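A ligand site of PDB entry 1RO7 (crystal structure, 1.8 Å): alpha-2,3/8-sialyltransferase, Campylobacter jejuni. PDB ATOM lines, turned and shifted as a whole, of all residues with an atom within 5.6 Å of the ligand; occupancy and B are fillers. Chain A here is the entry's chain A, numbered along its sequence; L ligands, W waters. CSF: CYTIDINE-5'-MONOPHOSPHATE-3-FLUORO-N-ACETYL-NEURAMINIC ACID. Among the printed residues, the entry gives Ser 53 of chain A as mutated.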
ATOM      1  N   GLY A   8       9.335  -0.775 -14.988  1.00  0.00           N
ATOM      2  CA  GLY A   8       8.022  -0.653 -14.400  1.00  0.00           C
ATOM      3  C   GLY A   8       8.259   0.387 -13.321  1.00  0.00           C
ATOM      4  O   GLY A   8       9.345   0.976 -13.276  1.00  0.00           O
ATOM      5  N   ASN A   9       7.305   0.608 -12.435  1.00  0.00           N
ATOM      6  CA  ASN A   9       7.501   1.596 -11.393  1.00  0.00           C
ATOM      7  C   ASN A   9       7.498   1.028  -9.981  1.00  0.00           C
ATOM      8  O   ASN A   9       7.268   1.756  -9.003  1.00  0.00           O
ATOM      9  CB  ASN A   9       6.478   2.721 -11.546  1.00  0.00           C
ATOM     10  CG  ASN A   9       6.626   3.450 -12.872  1.00  0.00           C
ATOM     11  OD1 ASN A   9       7.740   3.696 -13.329  1.00  0.00           O
ATOM     12  ND2 ASN A   9       5.511   3.784 -13.506  1.00  0.00           N
ATOM     13  N   GLY A  10       7.758  -0.265  -9.878  1.00  0.00           N
ATOM     14  CA  GLY A  10       7.798  -0.907  -8.576  1.00  0.00           C
ATOM     15  C   GLY A  10       8.970  -0.397  -7.760  1.00  0.00           C
ATOM     16  O   GLY A  10       9.837   0.286  -8.298  1.00  0.00           O
ATOM     17  N   PRO A  11       9.021  -0.709  -6.458  1.00  0.00           N
ATOM     18  CA  PRO A  11      10.110  -0.239  -5.592  1.00  0.00           C
ATOM     19  C   PRO A  11      11.515  -0.658  -6.019  1.00  0.00           C
ATOM     20  O   PRO A  11      12.500  -0.063  -5.566  1.00  0.00           O
ATOM     21  CB  PRO A  11       9.730  -0.784  -4.218  1.00  0.00           C
ATOM     22  CG  PRO A  11       8.963  -2.007  -4.543  1.00  0.00           C
ATOM     23  CD  PRO A  11       8.096  -1.560  -5.699  1.00  0.00           C
ATOM     24  N   CYS A  30       6.773   3.930 -18.314  1.00  0.00           N
ATOM     25  CA  CYS A  30       5.325   3.834 -18.400  1.00  0.00           C
ATOM     26  C   CYS A  30       4.621   4.593 -17.296  1.00  0.00           C
ATOM     27  O   CYS A  30       5.201   4.908 -16.260  1.00  0.00           O
ATOM     28  CB  CYS A  30       4.859   2.381 -18.370  1.00  0.00           C
ATOM     29  SG  CYS A  30       5.062   1.543 -16.762  1.00  0.00           S
ATOM     30  N   ASN A  31       3.355   4.900 -17.568  1.00  0.00           N
ATOM     31  CA  ASN A  31       2.471   5.553 -16.634  1.00  0.00           C
ATOM     32  C   ASN A  31       3.049   6.686 -15.776  1.00  0.00           C
ATOM     33  O   ASN A  31       3.477   7.705 -16.323  1.00  0.00           O
ATOM     34  CB  ASN A  31       1.822   4.470 -15.759  1.00  0.00           C
ATOM     35  CG  ASN A  31       1.212   3.362 -16.607  1.00  0.00           C
ATOM     36  OD1 ASN A  31       0.747   3.615 -17.726  1.00  0.00           O
ATOM     37  ND2 ASN A  31       1.181   2.152 -16.075  1.00  0.00           N
ATOM     38  N   GLN A  32       3.066   6.534 -14.460  1.00  0.00           N
ATOM     39  CA  GLN A  32       3.590   7.591 -13.607  1.00  0.00           C
ATOM     40  C   GLN A  32       5.094   7.533 -13.345  1.00  0.00           C
ATOM     41  O   GLN A  32       5.539   7.742 -12.219  1.00  0.00           O
ATOM     42  CB  GLN A  32       2.841   7.639 -12.271  1.00  0.00           C
ATOM     43  CG  GLN A  32       1.393   8.101 -12.358  1.00  0.00           C
ATOM     44  CD  GLN A  32       0.460   7.048 -12.933  1.00  0.00           C
ATOM     45  OE1 GLN A  32      -0.061   7.195 -14.037  1.00  0.00           O
ATOM     46  NE2 GLN A  32       0.261   5.966 -12.195  1.00  0.00           N
ATOM     47  N   ASN A  51      -1.753   4.010 -20.458  1.00  0.00           N
ATOM     48  CA  ASN A  51      -2.954   3.226 -20.644  1.00  0.00           C
ATOM     49  C   ASN A  51      -4.049   4.081 -21.277  1.00  0.00           C
ATOM     50  O   ASN A  51      -4.097   5.291 -21.091  1.00  0.00           O
ATOM     51  CB  ASN A  51      -3.447   2.672 -19.303  1.00  0.00           C
ATOM     52  CG  ASN A  51      -2.498   1.648 -18.714  1.00  0.00           C
ATOM     53  OD1 ASN A  51      -1.757   0.999 -19.449  1.00  0.00           O
ATOM     54  ND2 ASN A  51      -2.518   1.499 -17.396  1.00  0.00           N
ATOM     55  N   SER A  53      -7.149   4.435 -20.581  1.00  0.00           N
ATOM     56  CA  SER A  53      -7.982   5.095 -19.574  1.00  0.00           C
ATOM     57  C   SER A  53      -7.541   6.506 -19.187  1.00  0.00           C
ATOM     58  O   SER A  53      -8.381   7.360 -18.868  1.00  0.00           O
ATOM     59  CB  SER A  53      -8.052   4.234 -18.311  1.00  0.00           C
ATOM     60  OG  SER A  53      -6.780   4.134 -17.694  1.00  0.00           O
ATOM     61  N   LEU A  54      -6.245   6.750 -19.191  1.00  0.00           N
ATOM     62  CA  LEU A  54      -5.711   8.065 -18.822  1.00  0.00           C
ATOM     63  C   LEU A  54      -4.826   8.658 -19.905  1.00  0.00           C
ATOM     64  O   LEU A  54      -4.084   9.602 -19.644  1.00  0.00           O
ATOM     65  CB  LEU A  54      -4.906   7.948 -17.521  1.00  0.00           C
ATOM     66  CG  LEU A  54      -5.699   7.511 -16.274  1.00  0.00           C
ATOM     67  CD1 LEU A  54      -4.801   7.546 -15.060  1.00  0.00           C
ATOM     68  CD2 LEU A  54      -6.885   8.443 -16.080  1.00  0.00           C
ATOM     69  N   GLN A  58      -2.437  11.885 -19.648  1.00  0.00           N
ATOM     70  CA  GLN A  58      -1.003  11.604 -19.656  1.00  0.00           C
ATOM     71  C   GLN A  58      -0.311  12.315 -20.831  1.00  0.00           C
ATOM     72  O   GLN A  58       0.825  12.760 -20.703  1.00  0.00           O
ATOM     73  CB  GLN A  58      -0.748  10.095 -19.755  1.00  0.00           C
ATOM     74  CG  GLN A  58      -1.180   9.307 -18.520  1.00  0.00           C
ATOM     75  CD  GLN A  58      -0.202   9.424 -17.355  1.00  0.00           C
ATOM     76  OE1 GLN A  58       0.492  10.436 -17.193  1.00  0.00           O
ATOM     77  NE2 GLN A  58      -0.157   8.387 -16.525  1.00  0.00           N
ATOM     78  N   ILE A 130      -1.600  -9.567 -18.313  1.00  0.00           N
ATOM     79  CA  ILE A 130      -0.211  -9.162 -18.132  1.00  0.00           C
ATOM     80  C   ILE A 130      -0.224  -7.696 -17.694  1.00  0.00           C
ATOM     81  O   ILE A 130      -1.219  -6.997 -17.879  1.00  0.00           O
ATOM     82  CB  ILE A 130       0.590  -9.257 -19.461  1.00  0.00           C
ATOM     83  CG1 ILE A 130      -0.063  -8.377 -20.531  1.00  0.00           C
ATOM     84  CG2 ILE A 130       0.631 -10.700 -19.951  1.00  0.00           C
ATOM     85  CD1 ILE A 130       0.729  -8.293 -21.805  1.00  0.00           C
ATOM     86  N   THR A 131       0.881  -7.231 -17.098  1.00  0.00           N
ATOM     87  CA  THR A 131       0.978  -5.840 -16.674  1.00  0.00           C
ATOM     88  C   THR A 131       1.650  -5.070 -17.814  1.00  0.00           C
ATOM     89  O   THR A 131       2.158  -5.678 -18.750  1.00  0.00           O
ATOM     90  CB  THR A 131       1.841  -5.699 -15.398  1.00  0.00           C
ATOM     91  OG1 THR A 131       3.188  -6.073 -15.689  1.00  0.00           O
ATOM     92  CG2 THR A 131       1.296  -6.585 -14.278  1.00  0.00           C
ATOM     93  N   SER A 132       1.657  -3.739 -17.729  1.00  0.00           N
ATOM     94  CA  SER A 132       2.289  -2.941 -18.781  1.00  0.00           C
ATOM     95  C   SER A 132       3.786  -3.194 -18.886  1.00  0.00           C
ATOM     96  O   SER A 132       4.398  -2.947 -19.932  1.00  0.00           O
ATOM     97  CB  SER A 132       2.012  -1.453 -18.557  1.00  0.00           C
ATOM     98  OG  SER A 132       0.646  -1.165 -18.810  1.00  0.00           O
ATOM     99  N   GLY A 133       4.387  -3.662 -17.803  1.00  0.00           N
ATOM    100  CA  GLY A 133       5.803  -3.969 -17.851  1.00  0.00           C
ATOM    101  C   GLY A 133       6.011  -5.021 -18.916  1.00  0.00           C
ATOM    102  O   GLY A 133       6.938  -4.929 -19.723  1.00  0.00           O
ATOM    103  N   VAL A 134       5.135  -6.022 -18.942  1.00  0.00           N
ATOM    104  CA  VAL A 134       5.211  -7.105 -19.929  1.00  0.00           C
ATOM    105  C   VAL A 134       4.738  -6.624 -21.293  1.00  0.00           C
ATOM    106  O   VAL A 134       5.276  -7.032 -22.331  1.00  0.00           O
ATOM    107  CB  VAL A 134       4.361  -8.325 -19.487  1.00  0.00           C
ATOM    108  CG1 VAL A 134       4.451  -9.430 -20.529  1.00  0.00           C
ATOM    109  CG2 VAL A 134       4.852  -8.848 -18.143  1.00  0.00           C
ATOM    110  N   GLY A 152      12.112  -2.364 -12.011  1.00  0.00           N
ATOM    111  CA  GLY A 152      10.863  -1.820 -11.505  1.00  0.00           C
ATOM    112  C   GLY A 152       9.685  -2.774 -11.593  1.00  0.00           C
ATOM    113  O   GLY A 152       8.543  -2.361 -11.468  1.00  0.00           O
ATOM    114  N   ILE A 153       9.961  -4.052 -11.823  1.00  0.00           N
ATOM    115  CA  ILE A 153       8.898  -5.042 -11.901  1.00  0.00           C
ATOM    116  C   ILE A 153       8.958  -5.944 -10.670  1.00  0.00           C
ATOM    117  O   ILE A 153       9.848  -6.803 -10.565  1.00  0.00           O
ATOM    118  CB  ILE A 153       9.015  -5.882 -13.188  1.00  0.00           C
ATOM    119  CG1 ILE A 153       8.915  -4.965 -14.411  1.00  0.00           C
ATOM    120  CG2 ILE A 153       7.922  -6.947 -13.230  1.00  0.00           C
ATOM    121  CD1 ILE A 153       9.055  -5.664 -15.747  1.00  0.00           C
ATOM    122  N   ASP A 154       8.029  -5.751  -9.752  1.00  0.00           N
ATOM    123  CA  ASP A 154       8.019  -6.536  -8.527  1.00  0.00           C
ATOM    124  C   ASP A 154       6.753  -7.359  -8.281  1.00  0.00           C
ATOM    125  O   ASP A 154       6.588  -7.933  -7.210  1.00  0.00           O
ATOM    126  CB  ASP A 154       8.270  -5.613  -7.329  1.00  0.00           C
ATOM    127  CG  ASP A 154       9.619  -4.929  -7.409  1.00  0.00           C
ATOM    128  OD1 ASP A 154       9.703  -3.836  -8.016  1.00  0.00           O
ATOM    129  OD2 ASP A 154      10.603  -5.483  -6.869  1.00  0.00           O
ATOM    130  N   PHE A 155       5.883  -7.409  -9.283  1.00  0.00           N
ATOM    131  CA  PHE A 155       4.653  -8.199  -9.187  1.00  0.00           C
ATOM    132  C   PHE A 155       3.759  -7.796  -8.026  1.00  0.00           C
ATOM    133  O   PHE A 155       2.958  -8.593  -7.546  1.00  0.00           O
ATOM    134  CB  PHE A 155       5.010  -9.679  -9.046  1.00  0.00           C
ATOM    135  CG  PHE A 155       6.165 -10.108  -9.900  1.00  0.00           C
ATOM    136  CD1 PHE A 155       6.063 -10.106 -11.286  1.00  0.00           C
ATOM    137  CD2 PHE A 155       7.369 -10.501  -9.319  1.00  0.00           C
ATOM    138  CE1 PHE A 155       7.140 -10.478 -12.079  1.00  0.00           C
ATOM    139  CE2 PHE A 155       8.456 -10.874 -10.104  1.00  0.00           C
ATOM    140  CZ  PHE A 155       8.347 -10.866 -11.490  1.00  0.00           C
ATOM    141  N   TYR A 156       3.885  -6.548  -7.574  1.00  0.00           N
ATOM    142  CA  TYR A 156       3.082  -6.052  -6.474  1.00  0.00           C
ATOM    143  C   TYR A 156       3.149  -6.994  -5.272  1.00  0.00           C
ATOM    144  O   TYR A 156       2.139  -7.312  -4.650  1.00  0.00           O
ATOM    145  CB  TYR A 156       1.622  -5.879  -6.904  1.00  0.00           C
ATOM    146  CG  TYR A 156       1.441  -4.972  -8.097  1.00  0.00           C
ATOM    147  CD1 TYR A 156       1.596  -5.454  -9.401  1.00  0.00           C
ATOM    148  CD2 TYR A 156       1.145  -3.620  -7.932  1.00  0.00           C
ATOM    149  CE1 TYR A 156       1.455  -4.609 -10.497  1.00  0.00           C
ATOM    150  CE2 TYR A 156       1.008  -2.769  -9.020  1.00  0.00           C
ATOM    151  CZ  TYR A 156       1.163  -3.264 -10.303  1.00  0.00           C
ATOM    152  OH  TYR A 156       1.049  -2.417 -11.387  1.00  0.00           O
ATOM    153  N   GLN A 157       4.366  -7.440  -4.941  1.00  0.00           N
ATOM    154  CA  GLN A 157       4.577  -8.339  -3.829  1.00  0.00           C
ATOM    155  C   GLN A 157       4.161  -7.709  -2.504  1.00  0.00           C
ATOM    156  O   GLN A 157       3.429  -8.309  -1.712  1.00  0.00           O
ATOM    157  CB  GLN A 157       6.046  -8.767  -3.772  1.00  0.00           C
ATOM    158  CG  GLN A 157       7.036  -7.614  -3.880  1.00  0.00           C
ATOM    159  CD  GLN A 157       8.473  -8.088  -3.995  1.00  0.00           C
ATOM    160  OE1 GLN A 157       9.009  -8.714  -3.086  1.00  0.00           O
ATOM    161  NE2 GLN A 157       9.100  -7.791  -5.130  1.00  0.00           N
ATOM    162  N   GLY A 159       2.179  -5.380  -2.131  1.00  0.00           N
ATOM    163  CA  GLY A 159       0.960  -4.658  -2.409  1.00  0.00           C
ATOM    164  C   GLY A 159       1.142  -3.669  -3.548  1.00  0.00           C
ATOM    165  O   GLY A 159       1.837  -3.951  -4.521  1.00  0.00           O
ATOM    166  N   SER A 160       0.492  -2.510  -3.432  1.00  0.00           N
ATOM    167  CA  SER A 160       0.573  -1.482  -4.464  1.00  0.00           C
ATOM    168  C   SER A 160       1.714  -0.510  -4.181  1.00  0.00           C
ATOM    169  O   SER A 160       1.538   0.698  -4.266  1.00  0.00           O
ATOM    170  CB  SER A 160      -0.744  -0.720  -4.534  1.00  0.00           C
ATOM    171  OG  SER A 160      -1.819  -1.601  -4.803  1.00  0.00           O
ATOM    172  N   SER A 161       2.881  -1.043  -3.861  1.00  0.00           N
ATOM    173  CA  SER A 161       4.039  -0.218  -3.581  1.00  0.00           C
ATOM    174  C   SER A 161       4.677   0.296  -4.871  1.00  0.00           C
ATOM    175  O   SER A 161       4.521  -0.319  -5.929  1.00  0.00           O
ATOM    176  CB  SER A 161       5.082  -1.018  -2.797  1.00  0.00           C
ATOM    177  OG  SER A 161       5.504  -2.145  -3.529  1.00  0.00           O
ATOM    178  N   TYR A 162       5.365   1.428  -4.770  1.00  0.00           N
ATOM    179  CA  TYR A 162       6.040   2.018  -5.923  1.00  0.00           C
ATOM    180  C   TYR A 162       7.385   2.572  -5.514  1.00  0.00           C
ATOM    181  O   TYR A 162       7.738   2.596  -4.332  1.00  0.00           O
ATOM    182  CB  TYR A 162       5.197   3.142  -6.534  1.00  0.00           C
ATOM    183  CG  TYR A 162       3.931   2.644  -7.165  1.00  0.00           C
ATOM    184  CD1 TYR A 162       2.783   2.449  -6.396  1.00  0.00           C
ATOM    185  CD2 TYR A 162       3.898   2.305  -8.515  1.00  0.00           C
ATOM    186  CE1 TYR A 162       1.635   1.911  -6.966  1.00  0.00           C
ATOM    187  CE2 TYR A 162       2.754   1.756  -9.092  1.00  0.00           C
ATOM    188  CZ  TYR A 162       1.620   1.565  -8.307  1.00  0.00           C
ATOM    189  OH  TYR A 162       0.497   1.012  -8.851  1.00  0.00           O
ATOM    190  N   LEU A 171      -3.909  12.331  -9.534  1.00  0.00           N
ATOM    191  CA  LEU A 171      -3.976  10.921  -9.897  1.00  0.00           C
ATOM    192  C   LEU A 171      -5.113  10.238  -9.151  1.00  0.00           C
ATOM    193  O   LEU A 171      -5.844   9.425  -9.728  1.00  0.00           O
ATOM    194  CB  LEU A 171      -2.654  10.215  -9.573  1.00  0.00           C
ATOM    195  CG  LEU A 171      -2.569   8.741  -9.999  1.00  0.00           C
ATOM    196  CD1 LEU A 171      -2.634   8.630 -11.519  1.00  0.00           C
ATOM    197  CD2 LEU A 171      -1.285   8.128  -9.478  1.00  0.00           C
ATOM    198  N   ALA A 175      -7.987   8.394 -11.114  1.00  0.00           N
ATOM    199  CA  ALA A 175      -8.000   6.940 -10.953  1.00  0.00           C
ATOM    200  C   ALA A 175      -8.165   6.652  -9.471  1.00  0.00           C
ATOM    201  O   ALA A 175      -7.211   6.280  -8.793  1.00  0.00           O
ATOM    202  CB  ALA A 175      -6.684   6.361 -11.479  1.00  0.00           C
ATOM    203  N   ASN A 177      -9.045   4.241  -7.750  1.00  0.00           N
ATOM    204  CA  ASN A 177      -8.618   2.959  -7.197  1.00  0.00           C
ATOM    205  C   ASN A 177      -7.277   3.102  -6.474  1.00  0.00           C
ATOM    206  O   ASN A 177      -6.915   2.271  -5.636  1.00  0.00           O
ATOM    207  CB  ASN A 177      -8.527   1.903  -8.309  1.00  0.00           C
ATOM    208  CG  ASN A 177      -9.883   1.300  -8.657  1.00  0.00           C
ATOM    209  OD1 ASN A 177     -10.145   0.917  -9.802  1.00  0.00           O
ATOM    210  ND2 ASN A 177     -10.761   1.199  -7.662  1.00  0.00           N
ATOM    211  N   PHE A 178      -6.545   4.164  -6.777  1.00  0.00           N
ATOM    212  CA  PHE A 178      -5.262   4.398  -6.124  1.00  0.00           C
ATOM    213  C   PHE A 178      -5.437   4.763  -4.649  1.00  0.00           C
ATOM    214  O   PHE A 178      -4.489   4.700  -3.875  1.00  0.00           O
ATOM    215  CB  PHE A 178      -4.480   5.501  -6.854  1.00  0.00           C
ATOM    216  CG  PHE A 178      -3.682   5.003  -8.027  1.00  0.00           C
ATOM    217  CD1 PHE A 178      -2.546   4.237  -7.835  1.00  0.00           C
ATOM    218  CD2 PHE A 178      -4.091   5.294  -9.322  1.00  0.00           C
ATOM    219  CE1 PHE A 178      -1.801   3.769  -8.915  1.00  0.00           C
ATOM    220  CE2 PHE A 178      -3.367   4.829 -10.419  1.00  0.00           C
ATOM    221  CZ  PHE A 178      -2.211   4.072 -10.217  1.00  0.00           C
ATOM    222  N   SER A 183      -4.324  -1.254  -4.492  1.00  0.00           N
ATOM    223  CA  SER A 183      -4.881  -0.889  -5.794  1.00  0.00           C
ATOM    224  C   SER A 183      -4.501  -1.876  -6.901  1.00  0.00           C
ATOM    225  O   SER A 183      -4.889  -1.694  -8.060  1.00  0.00           O
ATOM    226  CB  SER A 183      -4.434   0.520  -6.180  1.00  0.00           C
ATOM    227  OG  SER A 183      -3.022   0.603  -6.222  1.00  0.00           O
ATOM    228  N   HIS A 184      -3.744  -2.908  -6.551  1.00  0.00           N
ATOM    229  CA  HIS A 184      -3.318  -3.913  -7.514  1.00  0.00           C
ATOM    230  C   HIS A 184      -4.532  -4.571  -8.192  1.00  0.00           C
ATOM    231  O   HIS A 184      -5.512  -4.894  -7.530  1.00  0.00           O
ATOM    232  CB  HIS A 184      -2.447  -4.959  -6.788  1.00  0.00           C
ATOM    233  CG  HIS A 184      -2.451  -6.308  -7.432  1.00  0.00           C
ATOM    234  ND1 HIS A 184      -3.496  -7.202  -7.289  1.00  0.00           N
ATOM    235  CD2 HIS A 184      -1.521  -6.946  -8.194  1.00  0.00           C
ATOM    236  CE1 HIS A 184      -3.205  -8.326  -7.927  1.00  0.00           C
ATOM    237  NE2 HIS A 184      -2.018  -8.193  -8.484  1.00  0.00           N
ATOM    238  N   TYR A 185      -4.456  -4.737  -9.512  1.00  0.00           N
ATOM    239  CA  TYR A 185      -5.553  -5.351 -10.269  1.00  0.00           C
ATOM    240  C   TYR A 185      -5.554  -6.869 -10.124  1.00  0.00           C
ATOM    241  O   TYR A 185      -4.574  -7.540 -10.456  1.00  0.00           O
ATOM    242  CB  TYR A 185      -5.455  -4.957 -11.752  1.00  0.00           C
ATOM    243  CG  TYR A 185      -6.498  -5.618 -12.617  1.00  0.00           C
ATOM    244  CD1 TYR A 185      -6.164  -6.665 -13.475  1.00  0.00           C
ATOM    245  CD2 TYR A 185      -7.841  -5.227 -12.554  1.00  0.00           C
ATOM    246  CE1 TYR A 185      -7.140  -7.297 -14.250  1.00  0.00           C
ATOM    247  CE2 TYR A 185      -8.813  -5.853 -13.321  1.00  0.00           C
ATOM    248  CZ  TYR A 185      -8.459  -6.892 -14.168  1.00  0.00           C
ATOM    249  OH  TYR A 185      -9.424  -7.537 -14.913  1.00  0.00           O
ATOM    250  N   HIS A 188      -3.906  -9.392 -12.479  1.00  0.00           N
ATOM    251  CA  HIS A 188      -2.448  -9.479 -12.584  1.00  0.00           C
ATOM    252  C   HIS A 188      -1.942 -10.502 -11.586  1.00  0.00           C
ATOM    253  O   HIS A 188      -2.563 -10.730 -10.547  1.00  0.00           O
ATOM    254  CB  HIS A 188      -1.792  -8.127 -12.279  1.00  0.00           C
ATOM    255  CG  HIS A 188      -2.161  -7.033 -13.231  1.00  0.00           C
ATOM    256  ND1 HIS A 188      -2.104  -7.182 -14.603  1.00  0.00           N
ATOM    257  CD2 HIS A 188      -2.556  -5.754 -13.012  1.00  0.00           C
ATOM    258  CE1 HIS A 188      -2.439  -6.042 -15.182  1.00  0.00           C
ATOM    259  NE2 HIS A 188      -2.722  -5.167 -14.236  1.00  0.00           N
ATOM    260  N   ASP A 193       2.696 -12.755 -15.313  1.00  0.00           N
ATOM    261  CA  ASP A 193       3.763 -11.979 -15.923  1.00  0.00           C
ATOM    262  C   ASP A 193       4.988 -12.839 -16.230  1.00  0.00           C
ATOM    263  O   ASP A 193       5.544 -12.781 -17.320  1.00  0.00           O
ATOM    264  CB  ASP A 193       4.157 -10.793 -15.043  1.00  0.00           C
ATOM    265  CG  ASP A 193       3.246  -9.578 -15.239  1.00  0.00           C
ATOM    266  OD1 ASP A 193       3.565  -8.507 -14.683  1.00  0.00           O
ATOM    267  OD2 ASP A 193       2.226  -9.692 -15.945  1.00  0.00           O
HETATM  268  C5A CSF L   1      -2.902   0.010 -12.409  1.00  0.00           C
HETATM  269  C4A CSF L   1      -1.982  -1.186 -12.153  1.00  0.00           C
HETATM  270  C2A CSF L   1      -0.907  -0.714 -14.507  1.00  0.00           C
HETATM  271  O6A CSF L   1      -1.372   0.636 -14.290  1.00  0.00           O
HETATM  272  C6A CSF L   1      -2.027   1.105 -13.074  1.00  0.00           C
HETATM  273  C3A CSF L   1      -1.347  -1.781 -13.470  1.00  0.00           C
HETATM  274  O4A CSF L   1      -2.823  -2.189 -11.537  1.00  0.00           O
HETATM  275  N5A CSF L   1      -3.499   0.592 -11.266  1.00  0.00           N
HETATM  276  C7A CSF L   1      -2.669   2.386 -13.634  1.00  0.00           C
HETATM  277  C8A CSF L   1      -1.847   3.435 -14.309  1.00  0.00           C
HETATM  278  C9A CSF L   1      -2.557   4.773 -14.583  1.00  0.00           C
HETATM  279  O9A CSF L   1      -1.781   5.584 -15.404  1.00  0.00           O
HETATM  280  O8A CSF L   1      -0.698   3.823 -13.544  1.00  0.00           O
HETATM  281  O7A CSF L   1      -3.746   1.970 -14.539  1.00  0.00           O
HETATM  282  C1A CSF L   1      -0.267  -1.157 -15.746  1.00  0.00           C
HETATM  283  OBA CSF L   1       0.374  -2.347 -15.800  1.00  0.00           O
HETATM  284  OAA CSF L   1      -0.373  -0.445 -16.684  1.00  0.00           O
HETATM  285  O1A CSF L   1       0.424  -0.498 -13.827  1.00  0.00           O
HETATM  286  O2A CSF L   1       0.885   0.448 -11.382  1.00  0.00           O
HETATM  287  N1  CSF L   1       5.013  -2.836 -10.979  1.00  0.00           N
HETATM  288  C2  CSF L   1       5.252  -4.137 -10.356  1.00  0.00           C
HETATM  289  N3  CSF L   1       5.087  -4.202  -8.901  1.00  0.00           N
HETATM  290  C4  CSF L   1       4.716  -3.088  -8.133  1.00  0.00           C
HETATM  291  C5  CSF L   1       4.457  -1.737  -8.778  1.00  0.00           C
HETATM  292  C6  CSF L   1       4.625  -1.688 -10.161  1.00  0.00           C
HETATM  293  C3' CSF L   1       3.312  -2.398 -13.974  1.00  0.00           C
HETATM  294  C2' CSF L   1       4.199  -3.466 -13.418  1.00  0.00           C
HETATM  295  C1' CSF L   1       5.199  -2.745 -12.522  1.00  0.00           C
HETATM  296  O4' CSF L   1       5.195  -1.362 -12.946  1.00  0.00           O
HETATM  297  C4' CSF L   1       4.268  -1.185 -14.042  1.00  0.00           C
HETATM  298  PA  CSF L   1       1.339   0.435 -12.800  1.00  0.00           P
HETATM  299  O5' CSF L   1       2.878   0.196 -12.604  1.00  0.00           O
HETATM  300  C5' CSF L   1       3.594   0.107 -13.861  1.00  0.00           C
HETATM  301  O3' CSF L   1       2.886  -2.691 -15.308  1.00  0.00           O
HETATM  302  O2' CSF L   1       4.974  -4.132 -14.435  1.00  0.00           O
HETATM  303  N4  CSF L   1       4.578  -3.223  -6.848  1.00  0.00           N
HETATM  304  O2  CSF L   1       5.601  -5.184 -11.018  1.00  0.00           O
HETATM  305  O3A CSF L   1       1.322   1.777 -13.192  1.00  0.00           O
HETATM  306  C10 CSF L   1      -4.732   1.131 -11.130  1.00  0.00           C
HETATM  307  O10 CSF L   1      -5.517   1.169 -12.086  1.00  0.00           O
HETATM  308  C11 CSF L   1      -5.116   1.681  -9.782  1.00  0.00           C
HETATM  309  F3A CSF L   1      -2.340  -2.354 -14.224  1.00  0.00           F
HETATM  310  O   HOH W   1       4.208  -7.279 -12.106  1.00  0.00           O
HETATM  311  O   HOH W   2      -7.547   2.861 -12.524  1.00  0.00           O
HETATM  312  O   HOH W   3      -2.169   0.108  -8.747  1.00  0.00           O
HETATM  313  O   HOH W   4       6.081  -4.624  -4.707  1.00  0.00           O
HETATM  314  O   HOH W   5       3.020   4.031 -12.529  1.00  0.00           O
HETATM  315  O   HOH W   6      -1.130   5.611 -18.072  1.00  0.00           O
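OBA of the ligand sits at hydrogen-bond distance from N of Ser 132 (2.7 Å). The side-chain hydroxyl of Ser 132 is in hydrogen-bond range of an oxygen (OAA) of the ligand. OH of Tyr 162 sits at hydrogen-bond distance from O2A of the ligand, at 2.6 Å. The side-chain amide nitrogen of Gln 32 lies within hydrogen-bond range of an oxygen (O8A) of the ligand (2.7 Å). The backbone NH of Asp 154 is in hydrogen-bond range of an oxygen (O2) of the ligand (2.8 Å). The backbone NH (N) of Phe 155 sits at hydrogen-bond distance from an oxygen (O2) of the ligand. N of Tyr 156 is in hydrogen-bond range of N3 of the ligand, 3.0 Å away. O2A of the ligand lies within hydrogen-bond range of OH of Tyr 156. The side-chain amide nitrogen (ND2) of Asn 31 is in hydrogen-bond range of an oxygen (O3A) of the ligand (2.9 Å). The side-chain hydroxyl (OG1) of Thr 131 sits at hydrogen-bond distance from an oxygen (O2') of the ligand, at 2.9 Å. The backbone NH of Asn 9 sits at hydrogen-bond distance from an oxygen (O4') of the ligand. ND2 of Asn 51 is in hydrogen-bond range of OAA of the ligand, 3.0 Å away. N4 of the ligand sits at hydrogen-bond distance from O of Ser 161 (3.0 Å). An oxygen (O3') of the ligand lies within hydrogen-bond range of the backbone NH (N) of Gly 133. The side-chain amide nitrogen (NE2) of Gln 58 lies within hydrogen-bond range of an oxygen (O9A) of the ligand (3.4 Å).
OG of Ser 132 sits at hydrogen-bond distance from OD1 of Asn 51 (3.3 Å). The side-chain amide oxygen of Gln 32 sits at hydrogen-bond distance from the side-chain amide nitrogen of Gln 58. NE2 of Gln 157 sits close to OD2 of Asp 154 (3.3 Å). The backbone carbonyl oxygen of Ile 130 lies close to a ring nitrogen (ND1) of His 188 (3.4 Å). The side-chain hydroxyl of Thr 131 sits at hydrogen-bond distance from the side-chain carboxylate of Asp 193 (2.7 Å). The backbone NH (N) of Asn 9 lies within hydrogen-bond range of the backbone carbonyl oxygen (O) of Gly 152 (3.4 Å). The backbone carbonyl oxygen of Cys 30 sits at hydrogen-bond distance from the side-chain amide nitrogen of Asn 9, 3.0 Å away. The backbone NH of Ser 183 is in hydrogen-bond range of the side-chain hydroxyl of Ser 160, 2.5 Å away.
A ring nitrogen (NE2) of His 188 sits close to a fluorine (F3A) of the ligand, at 2.8 Å. Gly 8 touches the ligand. CA of Gly 10 touches C5 of the ligand, at 3.4 Å. SG of Cys 30 touches C5' of the ligand, at 3.6 Å. Leu 54 touches the ligand. Gly 152 touches the ligand. Ile 153 touches the ligand (CA to O2, 3.4 Å). O of Gly 159 touches N4 of the ligand, 3.7 Å away. Asn 177 touches the ligand (CB to C11, 3.7 Å). Phe 178 touches the ligand. O of Ser 183 touches C11 of the ligand (3.8 Å). Tyr 185 touches the ligand. Of the 35 residues printed, 25 come within 4 Å of the ligand. The nearest printed residue that does not touch the ligand is Pro 11 (4.1 Å).
Water W1 lies within hydrogen-bond range of O2 of the ligand (2.7 Å), OD1 of Asp 193 (2.9 Å) and N of Phe 155 (3.3 Å). Water W6 lies within hydrogen-bond range of O9A of the ligand, OD1 of Asn 31, N of Asn 51 and NE2 of Gln 58. Water W3 lies within hydrogen-bond range of OG of Ser 183 (2.7 Å), OH of Tyr 162 (2.8 Å) and N5A of the ligand (2.9 Å). Water W5 lies within hydrogen-bond range of the side-chain amide nitrogen of Asn 9 (2.7 Å), an oxygen (O3A) of the ligand (2.9 Å) and the backbone NH of Gln 32 (3.2 Å). Water W4 lies within hydrogen-bond range of OG of Ser 161 (2.8 Å), N4 of the ligand (3.0 Å) and N of Gln 157 (3.3 Å).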
